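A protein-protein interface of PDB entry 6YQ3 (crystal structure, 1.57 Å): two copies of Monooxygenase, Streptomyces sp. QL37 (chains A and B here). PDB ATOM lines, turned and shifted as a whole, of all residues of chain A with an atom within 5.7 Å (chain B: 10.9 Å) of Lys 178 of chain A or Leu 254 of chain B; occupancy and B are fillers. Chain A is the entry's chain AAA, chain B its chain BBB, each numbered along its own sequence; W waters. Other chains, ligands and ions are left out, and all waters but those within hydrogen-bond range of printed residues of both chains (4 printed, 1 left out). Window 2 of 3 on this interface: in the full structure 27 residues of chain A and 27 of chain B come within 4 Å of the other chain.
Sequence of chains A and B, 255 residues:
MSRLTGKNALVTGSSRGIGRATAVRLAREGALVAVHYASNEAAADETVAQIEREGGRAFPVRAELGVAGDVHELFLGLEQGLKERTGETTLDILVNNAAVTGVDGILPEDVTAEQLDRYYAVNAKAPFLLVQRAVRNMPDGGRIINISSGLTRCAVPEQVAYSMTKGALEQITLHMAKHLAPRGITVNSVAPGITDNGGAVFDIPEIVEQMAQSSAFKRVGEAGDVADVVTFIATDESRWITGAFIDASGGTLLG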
ATOM      1  N   THR A 173       8.900  -7.276 -26.791  1.00  0.00           N
ATOM      2  CA  THR A 173       8.625  -8.448 -25.927  1.00  0.00           C
ATOM      3  C   THR A 173       9.873  -8.866 -25.162  1.00  0.00           C
ATOM      4  O   THR A 173       9.807  -8.989 -23.910  1.00  0.00           O
ATOM      5  CB  THR A 173       8.070  -9.614 -26.734  1.00  0.00           C
ATOM      6  OG1 THR A 173       6.778  -9.235 -27.228  1.00  0.00           O
ATOM      7  CG2 THR A 173       7.981 -10.867 -25.884  1.00  0.00           C
ATOM      8  N   LEU A 174      11.010  -9.029 -25.856  1.00  0.00           N
ATOM      9  CA  LEU A 174      12.182  -9.590 -25.222  1.00  0.00           C
ATOM     10  C   LEU A 174      12.609  -8.656 -24.091  1.00  0.00           C
ATOM     11  O   LEU A 174      12.898  -9.069 -22.951  1.00  0.00           O
ATOM     12  CB  LEU A 174      13.273  -9.801 -26.288  1.00  0.00           C
ATOM     13  CG  LEU A 174      14.588 -10.294 -25.714  1.00  0.00           C
ATOM     14  CD1 LEU A 174      14.430 -11.624 -24.963  1.00  0.00           C
ATOM     15  CD2 LEU A 174      15.604 -10.455 -26.808  1.00  0.00           C
ATOM     16  N   HIS A 175      12.895  -7.426 -24.484  1.00  0.00           N
ATOM     17  CA  HIS A 175      13.609  -6.482 -23.607  1.00  0.00           C
ATOM     18  C   HIS A 175      12.655  -5.946 -22.517  1.00  0.00           C
ATOM     19  O   HIS A 175      13.076  -5.807 -21.330  1.00  0.00           O
ATOM     20  CB  HIS A 175      14.256  -5.393 -24.454  1.00  0.00           C
ATOM     21  CG  HIS A 175      15.302  -5.918 -25.344  1.00  0.00           C
ATOM     22  ND1 HIS A 175      16.550  -6.309 -24.855  1.00  0.00           N
ATOM     23  CD2 HIS A 175      15.239  -6.245 -26.646  1.00  0.00           C
ATOM     24  CE1 HIS A 175      17.239  -6.822 -25.904  1.00  0.00           C
ATOM     25  NE2 HIS A 175      16.425  -6.838 -27.025  1.00  0.00           N
ATOM     26  N   MET A 176      11.397  -5.728 -22.833  1.00  0.00           N
ATOM     27  CA  MET A 176      10.453  -5.267 -21.797  1.00  0.00           C
ATOM     28  C   MET A 176      10.085  -6.404 -20.849  1.00  0.00           C
ATOM     29  O   MET A 176       9.785  -6.136 -19.673  1.00  0.00           O
ATOM     30  CB  MET A 176       9.204  -4.587 -22.374  1.00  0.00           C
ATOM     31  CG  MET A 176       9.507  -3.321 -23.205  1.00  0.00           C
ATOM     32  SD  MET A 176      10.406  -2.082 -22.227  1.00  0.00           S
ATOM     33  CE  MET A 176       9.157  -1.559 -21.056  1.00  0.00           C
ATOM     34  N   ALA A 177      10.092  -7.677 -21.257  1.00  0.00           N
ATOM     35  CA  ALA A 177       9.887  -8.771 -20.296  1.00  0.00           C
ATOM     36  C   ALA A 177      10.913  -8.726 -19.182  1.00  0.00           C
ATOM     37  O   ALA A 177      10.582  -8.801 -18.026  1.00  0.00           O
ATOM     38  CB  ALA A 177       9.942 -10.122 -21.031  1.00  0.00           C
ATOM     39  N   LYS A 178      12.173  -8.500 -19.547  1.00  0.00           N
ATOM     40  CA  LYS A 178      13.230  -8.405 -18.513  1.00  0.00           C
ATOM     41  C   LYS A 178      13.009  -7.160 -17.645  1.00  0.00           C
ATOM     42  O   LYS A 178      13.122  -7.231 -16.414  1.00  0.00           O
ATOM     43  CB  LYS A 178      14.587  -8.370 -19.202  1.00  0.00           C
ATOM     44  CG  LYS A 178      15.758  -8.286 -18.239  1.00  0.00           C
ATOM     45  CD  LYS A 178      15.920  -9.409 -17.313  1.00  0.00           C
ATOM     46  CE  LYS A 178      17.186  -9.290 -16.481  1.00  0.00           C
ATOM     47  NZ  LYS A 178      17.342 -10.517 -15.636  1.00  0.00           N
ATOM     48  N   HIS A 179      12.663  -6.040 -18.281  1.00  0.00           N
ATOM     49  CA  HIS A 179      12.537  -4.739 -17.584  1.00  0.00           C
ATOM     50  C   HIS A 179      11.399  -4.824 -16.562  1.00  0.00           C
ATOM     51  O   HIS A 179      11.531  -4.281 -15.472  1.00  0.00           O
ATOM     52  CB  HIS A 179      12.233  -3.633 -18.593  1.00  0.00           C
ATOM     53  CG  HIS A 179      12.205  -2.304 -17.944  1.00  0.00           C
ATOM     54  ND1 HIS A 179      13.346  -1.812 -17.358  1.00  0.00           N
ATOM     55  CD2 HIS A 179      11.232  -1.399 -17.814  1.00  0.00           C
ATOM     56  CE1 HIS A 179      13.024  -0.625 -16.864  1.00  0.00           C
ATOM     57  NE2 HIS A 179      11.783  -0.345 -17.133  1.00  0.00           N
ATOM     58  N   LEU A 180      10.308  -5.443 -16.935  1.00  0.00           N
ATOM     59  CA  LEU A 180       9.068  -5.420 -16.106  1.00  0.00           C
ATOM     60  C   LEU A 180       8.943  -6.631 -15.175  1.00  0.00           C
ATOM     61  O   LEU A 180       8.021  -6.646 -14.347  1.00  0.00           O
ATOM     62  CB  LEU A 180       7.848  -5.297 -17.008  1.00  0.00           C
ATOM     63  CG  LEU A 180       7.810  -4.001 -17.815  1.00  0.00           C
ATOM     64  CD1 LEU A 180       6.707  -4.063 -18.809  1.00  0.00           C
ATOM     65  CD2 LEU A 180       7.607  -2.757 -16.937  1.00  0.00           C
ATOM     66  N   ALA A 181       9.831  -7.624 -15.288  1.00  0.00           N
ATOM     67  CA  ALA A 181       9.793  -8.828 -14.447  1.00  0.00           C
ATOM     68  C   ALA A 181       9.736  -8.487 -12.939  1.00  0.00           C
ATOM     69  O   ALA A 181       8.933  -9.098 -12.197  1.00  0.00           O
ATOM     70  CB  ALA A 181      10.938  -9.727 -14.776  1.00  0.00           C
ATOM     71  N   PRO A 182      10.478  -7.456 -12.455  1.00  0.00           N
ATOM     72  CA  PRO A 182      10.457  -7.126 -11.027  1.00  0.00           C
ATOM     73  C   PRO A 182       9.080  -6.734 -10.549  1.00  0.00           C
ATOM     74  O   PRO A 182       8.827  -6.733  -9.329  1.00  0.00           O
ATOM     75  CB  PRO A 182      11.468  -5.981 -10.901  1.00  0.00           C
ATOM     76  CG  PRO A 182      12.420  -6.233 -12.061  1.00  0.00           C
ATOM     77  CD  PRO A 182      11.515  -6.704 -13.178  1.00  0.00           C
ATOM     78  N   THR A 242       7.009 -15.532 -19.774  1.00  0.00           N
ATOM     79  CA  THR A 242       7.343 -14.145 -20.106  1.00  0.00           C
ATOM     80  C   THR A 242       8.488 -14.130 -21.097  1.00  0.00           C
ATOM     81  O   THR A 242       9.352 -15.004 -21.080  1.00  0.00           O
ATOM     82  CB  THR A 242       7.591 -13.350 -18.835  1.00  0.00           C
ATOM     83  OG1 THR A 242       7.471 -11.958 -19.204  1.00  0.00           O
ATOM     84  CG2 THR A 242       8.947 -13.621 -18.251  1.00  0.00           C
ATOM     85  N   GLY A 243       8.444 -13.095 -21.919  1.00  0.00           N
ATOM     86  CA  GLY A 243       9.455 -12.902 -22.951  1.00  0.00           C
ATOM     87  C   GLY A 243       9.360 -13.902 -24.040  1.00  0.00           C
ATOM     88  O   GLY A 243      10.352 -14.056 -24.767  1.00  0.00           O
ATOM     89  N   GLY B 150      14.544 -25.707 -20.342  1.00  0.00           N
ATOM     90  CA  GLY B 150      15.242 -24.531 -20.831  1.00  0.00           C
ATOM     91  C   GLY B 150      16.693 -24.783 -21.123  1.00  0.00           C
ATOM     92  O   GLY B 150      17.227 -23.983 -21.873  1.00  0.00           O
ATOM     93  N   LEU B 151      17.257 -25.893 -20.635  1.00  0.00           N
ATOM     94  CA  LEU B 151      18.667 -26.225 -20.967  1.00  0.00           C
ATOM     95  C   LEU B 151      18.845 -26.503 -22.442  1.00  0.00           C
ATOM     96  O   LEU B 151      20.019 -26.502 -22.881  1.00  0.00           O
ATOM     97  CB  LEU B 151      19.129 -27.376 -20.111  1.00  0.00           C
ATOM     98  CG  LEU B 151      19.219 -27.052 -18.633  1.00  0.00           C
ATOM     99  CD1 LEU B 151      19.782 -28.254 -17.858  1.00  0.00           C
ATOM    100  CD2 LEU B 151      20.057 -25.828 -18.351  1.00  0.00           C
ATOM    101  N   ARG B 153      18.323 -24.375 -24.541  1.00  0.00           N
ATOM    102  CA  ARG B 153      18.618 -22.997 -24.993  1.00  0.00           C
ATOM    103  C   ARG B 153      19.620 -22.301 -24.078  1.00  0.00           C
ATOM    104  O   ARG B 153      19.928 -21.108 -24.365  1.00  0.00           O
ATOM    105  CB  ARG B 153      17.313 -22.199 -25.115  1.00  0.00           C
ATOM    106  CG  ARG B 153      16.369 -22.784 -26.164  1.00  0.00           C
ATOM    107  CD  ARG B 153      15.256 -21.881 -26.687  1.00  0.00           C
ATOM    108  NE  ARG B 153      14.425 -22.548 -27.672  1.00  0.00           N
ATOM    109  CZ  ARG B 153      13.478 -21.967 -28.375  1.00  0.00           C
ATOM    110  NH1 ARG B 153      13.274 -20.663 -28.256  1.00  0.00           N
ATOM    111  NH2 ARG B 153      12.828 -22.707 -29.255  1.00  0.00           N
ATOM    112  N   CYS B 154      20.128 -22.967 -23.053  1.00  0.00           N
ATOM    113  CA  CYS B 154      20.921 -22.350 -21.978  1.00  0.00           C
ATOM    114  C   CYS B 154      22.080 -23.292 -21.641  1.00  0.00           C
ATOM    115  O   CYS B 154      21.776 -24.366 -21.155  1.00  0.00           O
ATOM    116  CB  CYS B 154      20.039 -22.151 -20.742  1.00  0.00           C
ATOM    117  SG  CYS B 154      20.901 -21.166 -19.526  1.00  0.00           S
ATOM    118  N   ALA B 155      23.331 -22.908 -21.944  1.00  0.00           N
ATOM    119  CA  ALA B 155      24.451 -23.838 -21.807  1.00  0.00           C
ATOM    120  C   ALA B 155      24.770 -24.099 -20.349  1.00  0.00           C
ATOM    121  O   ALA B 155      25.005 -23.145 -19.581  1.00  0.00           O
ATOM    122  CB  ALA B 155      25.667 -23.275 -22.527  1.00  0.00           C
ATOM    123  N   ALA B 191       8.719 -26.097 -21.776  1.00  0.00           N
ATOM    124  CA  ALA B 191      10.092 -26.123 -21.245  1.00  0.00           C
ATOM    125  C   ALA B 191      10.104 -25.428 -19.914  1.00  0.00           C
ATOM    126  O   ALA B 191      10.034 -24.219 -19.832  1.00  0.00           O
ATOM    127  CB  ALA B 191      11.025 -25.392 -22.184  1.00  0.00           C
ATOM    128  N   GLY B 193      12.017 -24.077 -16.447  1.00  0.00           N
ATOM    129  CA  GLY B 193      13.314 -23.746 -15.871  1.00  0.00           C
ATOM    130  C   GLY B 193      13.521 -24.493 -14.563  1.00  0.00           C
ATOM    131  O   GLY B 193      12.888 -25.561 -14.358  1.00  0.00           O
ATOM    132  N   ALA B 212      17.423 -19.375  -7.842  1.00  0.00           N
ATOM    133  CA  ALA B 212      16.380 -18.336  -8.083  1.00  0.00           C
ATOM    134  C   ALA B 212      16.897 -17.279  -9.070  1.00  0.00           C
ATOM    135  O   ALA B 212      16.072 -16.684  -9.848  1.00  0.00           O
ATOM    136  CB  ALA B 212      15.944 -17.739  -6.778  1.00  0.00           C
ATOM    137  N   GLN B 213      18.214 -17.039  -9.108  1.00  0.00           N
ATOM    138  CA  GLN B 213      18.770 -15.926  -9.913  1.00  0.00           C
ATOM    139  C   GLN B 213      18.612 -16.205 -11.417  1.00  0.00           C
ATOM    140  O   GLN B 213      18.683 -15.243 -12.168  1.00  0.00           O
ATOM    141  CB  GLN B 213      20.233 -15.626  -9.545  1.00  0.00           C
ATOM    142  CG  GLN B 213      20.457 -15.322  -8.076  1.00  0.00           C
ATOM    143  CD  GLN B 213      19.459 -14.330  -7.509  1.00  0.00           C
ATOM    144  OE1 GLN B 213      19.344 -13.213  -8.006  1.00  0.00           O
ATOM    145  NE2 GLN B 213      18.755 -14.710  -6.451  1.00  0.00           N
ATOM    146  N   SER B 214      18.389 -17.461 -11.807  1.00  0.00           N
ATOM    147  CA  SER B 214      18.284 -17.884 -13.218  1.00  0.00           C
ATOM    148  C   SER B 214      16.969 -17.318 -13.782  1.00  0.00           C
ATOM    149  O   SER B 214      16.937 -17.024 -15.003  1.00  0.00           O
ATOM    150  CB  SER B 214      18.456 -19.382 -13.425  1.00  0.00           C
ATOM    151  OG  SER B 214      17.419 -20.146 -12.816  1.00  0.00           O
ATOM    152  N   SER B 215      15.931 -17.153 -12.958  1.00  0.00           N
ATOM    153  CA  SER B 215      14.612 -16.678 -13.432  1.00  0.00           C
ATOM    154  C   SER B 215      14.613 -15.153 -13.456  1.00  0.00           C
ATOM    155  O   SER B 215      15.155 -14.502 -12.499  1.00  0.00           O
ATOM    156  CB  SER B 215      13.459 -17.210 -12.554  1.00  0.00           C
ATOM    157  OG  SER B 215      12.303 -16.400 -12.733  1.00  0.00           O
ATOM    158  N   ALA B 216      13.918 -14.526 -14.410  1.00  0.00           N
ATOM    159  CA  ALA B 216      13.780 -13.049 -14.421  1.00  0.00           C
ATOM    160  C   ALA B 216      13.013 -12.568 -13.167  1.00  0.00           C
ATOM    161  O   ALA B 216      13.158 -11.388 -12.773  1.00  0.00           O
ATOM    162  CB  ALA B 216      13.090 -12.585 -15.702  1.00  0.00           C
ATOM    163  N   PHE B 217      12.186 -13.436 -12.576  1.00  0.00           N
ATOM    164  CA  PHE B 217      11.369 -13.143 -11.387  1.00  0.00           C
ATOM    165  C   PHE B 217      12.142 -13.402 -10.095  1.00  0.00           C
ATOM    166  O   PHE B 217      11.567 -13.155  -9.023  1.00  0.00           O
ATOM    167  CB  PHE B 217      10.078 -13.959 -11.445  1.00  0.00           C
ATOM    168  CG  PHE B 217       9.264 -13.605 -12.677  1.00  0.00           C
ATOM    169  CD1 PHE B 217       8.715 -12.347 -12.849  1.00  0.00           C
ATOM    170  CD2 PHE B 217       8.998 -14.560 -13.635  1.00  0.00           C
ATOM    171  CE1 PHE B 217       7.984 -12.036 -13.971  1.00  0.00           C
ATOM    172  CE2 PHE B 217       8.178 -14.272 -14.712  1.00  0.00           C
ATOM    173  CZ  PHE B 217       7.688 -13.008 -14.892  1.00  0.00           C
ATOM    174  N   LYS B 218      13.338 -13.938 -10.194  1.00  0.00           N
ATOM    175  CA  LYS B 218      14.247 -14.141  -9.027  1.00  0.00           C
ATOM    176  C   LYS B 218      13.568 -15.035  -7.987  1.00  0.00           C
ATOM    177  O   LYS B 218      13.717 -14.821  -6.784  1.00  0.00           O
ATOM    178  CB  LYS B 218      14.718 -12.801  -8.486  1.00  0.00           C
ATOM    179  CG  LYS B 218      15.446 -11.928  -9.517  1.00  0.00           C
ATOM    180  CD  LYS B 218      16.705 -12.500 -10.097  1.00  0.00           C
ATOM    181  CE  LYS B 218      17.092 -11.781 -11.378  1.00  0.00           C
ATOM    182  NZ  LYS B 218      18.326 -12.372 -11.968  1.00  0.00           N
ATOM    183  N   ARG B 219      12.852 -16.054  -8.479  1.00  0.00           N
ATOM    184  CA  ARG B 219      12.387 -17.169  -7.629  1.00  0.00           C
ATOM    185  C   ARG B 219      12.554 -18.445  -8.454  1.00  0.00           C
ATOM    186  O   ARG B 219      12.591 -18.390  -9.742  1.00  0.00           O
ATOM    187  CB  ARG B 219      10.960 -17.010  -7.124  1.00  0.00           C
ATOM    188  CG  ARG B 219       9.894 -16.951  -8.212  1.00  0.00           C
ATOM    189  CD  ARG B 219       8.502 -16.881  -7.576  1.00  0.00           C
ATOM    190  NE  ARG B 219       7.411 -16.907  -8.531  1.00  0.00           N
ATOM    191  CZ  ARG B 219       6.777 -18.003  -8.943  1.00  0.00           C
ATOM    192  NH1 ARG B 219       5.678 -17.888  -9.703  1.00  0.00           N
ATOM    193  NH2 ARG B 219       7.282 -19.190  -8.665  1.00  0.00           N
ATOM    194  N   PHE B 245       7.481 -24.589 -29.132  1.00  0.00           N
ATOM    195  CA  PHE B 245       8.302 -24.513 -27.908  1.00  0.00           C
ATOM    196  C   PHE B 245       7.624 -23.495 -26.994  1.00  0.00           C
ATOM    197  O   PHE B 245       7.598 -22.275 -27.320  1.00  0.00           O
ATOM    198  CB  PHE B 245       9.713 -24.115 -28.287  1.00  0.00           C
ATOM    199  CG  PHE B 245      10.601 -23.930 -27.081  1.00  0.00           C
ATOM    200  CD1 PHE B 245      11.317 -25.022 -26.603  1.00  0.00           C
ATOM    201  CD2 PHE B 245      10.733 -22.702 -26.447  1.00  0.00           C
ATOM    202  CE1 PHE B 245      12.167 -24.910 -25.523  1.00  0.00           C
ATOM    203  CE2 PHE B 245      11.636 -22.606 -25.375  1.00  0.00           C
ATOM    204  CZ  PHE B 245      12.363 -23.692 -24.945  1.00  0.00           C
ATOM    205  N   ASP B 247       7.670 -21.690 -23.553  1.00  0.00           N
ATOM    206  CA  ASP B 247       8.596 -21.308 -22.477  1.00  0.00           C
ATOM    207  C   ASP B 247       7.800 -21.182 -21.191  1.00  0.00           C
ATOM    208  O   ASP B 247       7.040 -20.246 -21.059  1.00  0.00           O
ATOM    209  CB  ASP B 247       9.337 -20.053 -22.869  1.00  0.00           C
ATOM    210  CG  ASP B 247      10.381 -19.620 -21.884  1.00  0.00           C
ATOM    211  OD1 ASP B 247      10.194 -19.837 -20.650  1.00  0.00           O
ATOM    212  OD2 ASP B 247      11.275 -18.850 -22.327  1.00  0.00           O
ATOM    213  N   ALA B 248       7.976 -22.131 -20.267  1.00  0.00           N
ATOM    214  CA  ALA B 248       7.356 -22.065 -18.933  1.00  0.00           C
ATOM    215  C   ALA B 248       8.459 -21.985 -17.872  1.00  0.00           C
ATOM    216  O   ALA B 248       8.560 -22.844 -16.976  1.00  0.00           O
ATOM    217  CB  ALA B 248       6.440 -23.251 -18.756  1.00  0.00           C
ATOM    218  N   SER B 249       9.413 -21.091 -18.086  1.00  0.00           N
ATOM    219  CA  SER B 249      10.660 -21.015 -17.279  1.00  0.00           C
ATOM    220  C   SER B 249      10.701 -19.809 -16.338  1.00  0.00           C
ATOM    221  O   SER B 249      11.775 -19.531 -15.743  1.00  0.00           O
ATOM    222  CB  SER B 249      11.869 -21.052 -18.184  1.00  0.00           C
ATOM    223  OG  SER B 249      12.047 -19.797 -18.859  1.00  0.00           O
ATOM    224  N   GLY B 250       9.648 -18.984 -16.261  1.00  0.00           N
ATOM    225  CA  GLY B 250       9.725 -17.756 -15.475  1.00  0.00           C
ATOM    226  C   GLY B 250      10.794 -16.834 -16.029  1.00  0.00           C
ATOM    227  O   GLY B 250      11.530 -16.212 -15.291  1.00  0.00           O
ATOM    228  N   GLY B 251      10.916 -16.726 -17.337  1.00  0.00           N
ATOM    229  CA  GLY B 251      11.861 -15.767 -17.944  1.00  0.00           C
ATOM    230  C   GLY B 251      13.328 -16.152 -17.722  1.00  0.00           C
ATOM    231  O   GLY B 251      14.192 -15.308 -17.605  1.00  0.00           O
ATOM    232  N   THR B 252      13.635 -17.420 -17.736  1.00  0.00           N
ATOM    233  CA  THR B 252      15.026 -17.916 -17.629  1.00  0.00           C
ATOM    234  C   THR B 252      15.758 -17.719 -18.945  1.00  0.00           C
ATOM    235  O   THR B 252      17.001 -17.657 -18.925  1.00  0.00           O
ATOM    236  CB  THR B 252      15.023 -19.403 -17.249  1.00  0.00           C
ATOM    237  OG1 THR B 252      14.365 -19.537 -15.985  1.00  0.00           O
ATOM    238  CG2 THR B 252      16.420 -19.968 -17.122  1.00  0.00           C
ATOM    239  N   LEU B 253      15.067 -17.709 -20.052  1.00  0.00           N
ATOM    240  CA  LEU B 253      15.712 -17.714 -21.401  1.00  0.00           C
ATOM    241  C   LEU B 253      15.783 -16.304 -21.979  1.00  0.00           C
ATOM    242  O   LEU B 253      15.469 -16.191 -23.269  1.00  0.00           O
ATOM    243  CB  LEU B 253      14.861 -18.558 -22.323  1.00  0.00           C
ATOM    244  CG  LEU B 253      14.715 -20.017 -21.891  1.00  0.00           C
ATOM    245  CD1 LEU B 253      13.969 -20.836 -22.952  1.00  0.00           C
ATOM    246  CD2 LEU B 253      16.060 -20.620 -21.532  1.00  0.00           C
ATOM    247  N   LEU B 254      15.948 -15.311 -21.147  1.00  0.00           N
ATOM    248  CA  LEU B 254      16.035 -13.901 -21.643  1.00  0.00           C
ATOM    249  C   LEU B 254      17.497 -13.652 -22.052  1.00  0.00           C
ATOM    250  O   LEU B 254      17.807 -12.601 -22.569  1.00  0.00           O
ATOM    251  CB  LEU B 254      15.462 -12.962 -20.570  1.00  0.00           C
ATOM    252  CG  LEU B 254      13.946 -13.134 -20.337  1.00  0.00           C
ATOM    253  CD1 LEU B 254      13.376 -12.099 -19.404  1.00  0.00           C
ATOM    254  CD2 LEU B 254      13.149 -13.063 -21.588  1.00  0.00           C
ATOM    255  N   GLY B 255      18.319 -14.714 -22.102  1.00  0.00           N
ATOM    256  CA  GLY B 255      19.701 -14.644 -22.630  1.00  0.00           C
ATOM    257  C   GLY B 255      20.668 -14.002 -21.654  1.00  0.00           C
ATOM    258  O   GLY B 255      21.863 -14.223 -21.987  1.00  0.00           O
HETATM  259  O   HOH W   1      17.635 -13.581 -14.493  1.00  0.00           O
HETATM  260  O   HOH W   2      12.147 -16.950 -20.895  1.00  0.00           O
HETATM  261  O   HOH W   3      15.153  -9.873 -13.774  1.00  0.00           O
HETATM  262  O   HOH W   4      12.661 -15.455 -24.287  1.00  0.00           O
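Among the printed residues, 7 pairs touch across the chains.
Among the printed residues, no Asp or Glu carboxylate lies within 4 Å of a Lys or Arg side-chain nitrogen of the other chain.
Water W2 lies within hydrogen-bond range of OD2 of Asp 247 of chain B (2.5 Å), N of Leu 253 of chain B (3.1 Å) and O of Thr 242 of chain A (3.4 Å).
Water W3 lies within hydrogen-bond range of O of Ala 216 of chain B (2.7 Å) and NZ of Lys 178 of chain A (2.9 Å).
Water W4 lies within hydrogen-bond range of O of Gly 243 of chain A (2.7 Å) and O of Leu 253 of chain B (3.1 Å).
Water W1 lies within hydrogen-bond range of the side-chain amino group of Lys 218 of chain B, the backbone carbonyl oxygen of Gln 213 of chain B, the side-chain amino group of Lys 178 of chain A and the backbone carbonyl oxygen of Ser 215 of chain B.
No position is printed for both chains.
Of the 7 pairs that touch across the chains among the printed residues, none has its exchanged pair printed and touching as well.
N of Phe 217 of chain B is in hydrogen-bond range of OG of Ser 215 of chain B (3.0 Å).
N of Ala 216 of chain B lies within hydrogen-bond range of O of Gly 250 of chain B (3.1 Å).
The backbone carbonyl oxygen of Gly 251 of chain B lies within hydrogen-bond range of the backbone NH of Ala 216 of chain B.
Leu 254 of chain B touches Leu 174 of chain A (CD2 to CD1, 3.9 Å).
CD1 of Leu 254 of chain B touches N of Lys 178 of chain A, at 3.8 Å.
Ala 181 of chain A touches Ala 216 of chain B (CB to O, 3.4 Å).
Ala 181 of chain A touches Phe 217 of chain B (O to CD1, 3.3 Å).
Thr 242 of chain A touches Phe 217 of chain B (CG2 to CZ, 3.6 Å).
Thr 242 of chain A touches Gly 251 of chain B.
CD2 of Leu 254 of chain B touches CA of Gly 243 of chain A, at 3.9 Å.
Leu 174 of chain A touches just one residue of chain B: Leu 254.
His 175 of chain A touches none of the printed residues of chain B.
No residue of chain B comes within 4 Å of Ala 177 of chain A.
Lys 178 of chain A touches just one residue of chain B: Leu 254 (3.8 Å).
Of chain B, only Ala 216 and Phe 217 come within 4 Å of Ala 181 of chain A.
Of the printed residues of chain B, Thr 242 of chain A touches Phe 217 and Gly 251.
Gly 243 of chain A touches just one residue of chain B: Leu 254.
Printed residues of chain A within 4 Å of Ala 216 of chain B: Ala 181 (3.4 Å).
Printed residues of chain A within 4 Å of Phe 217 of chain B: Ala 181 (3.3 Å) and Thr 242 (3.6 Å).
Thr 252 of chain B touches none of the printed residues of chain A.
Leu 254 of chain B touches just these residues of chain A: Leu 174, Lys 178 and Gly 243.
The nearest residue of chain A that does not touch Leu 254 of chain B is Ala 177 of chain A (4.2 Å).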
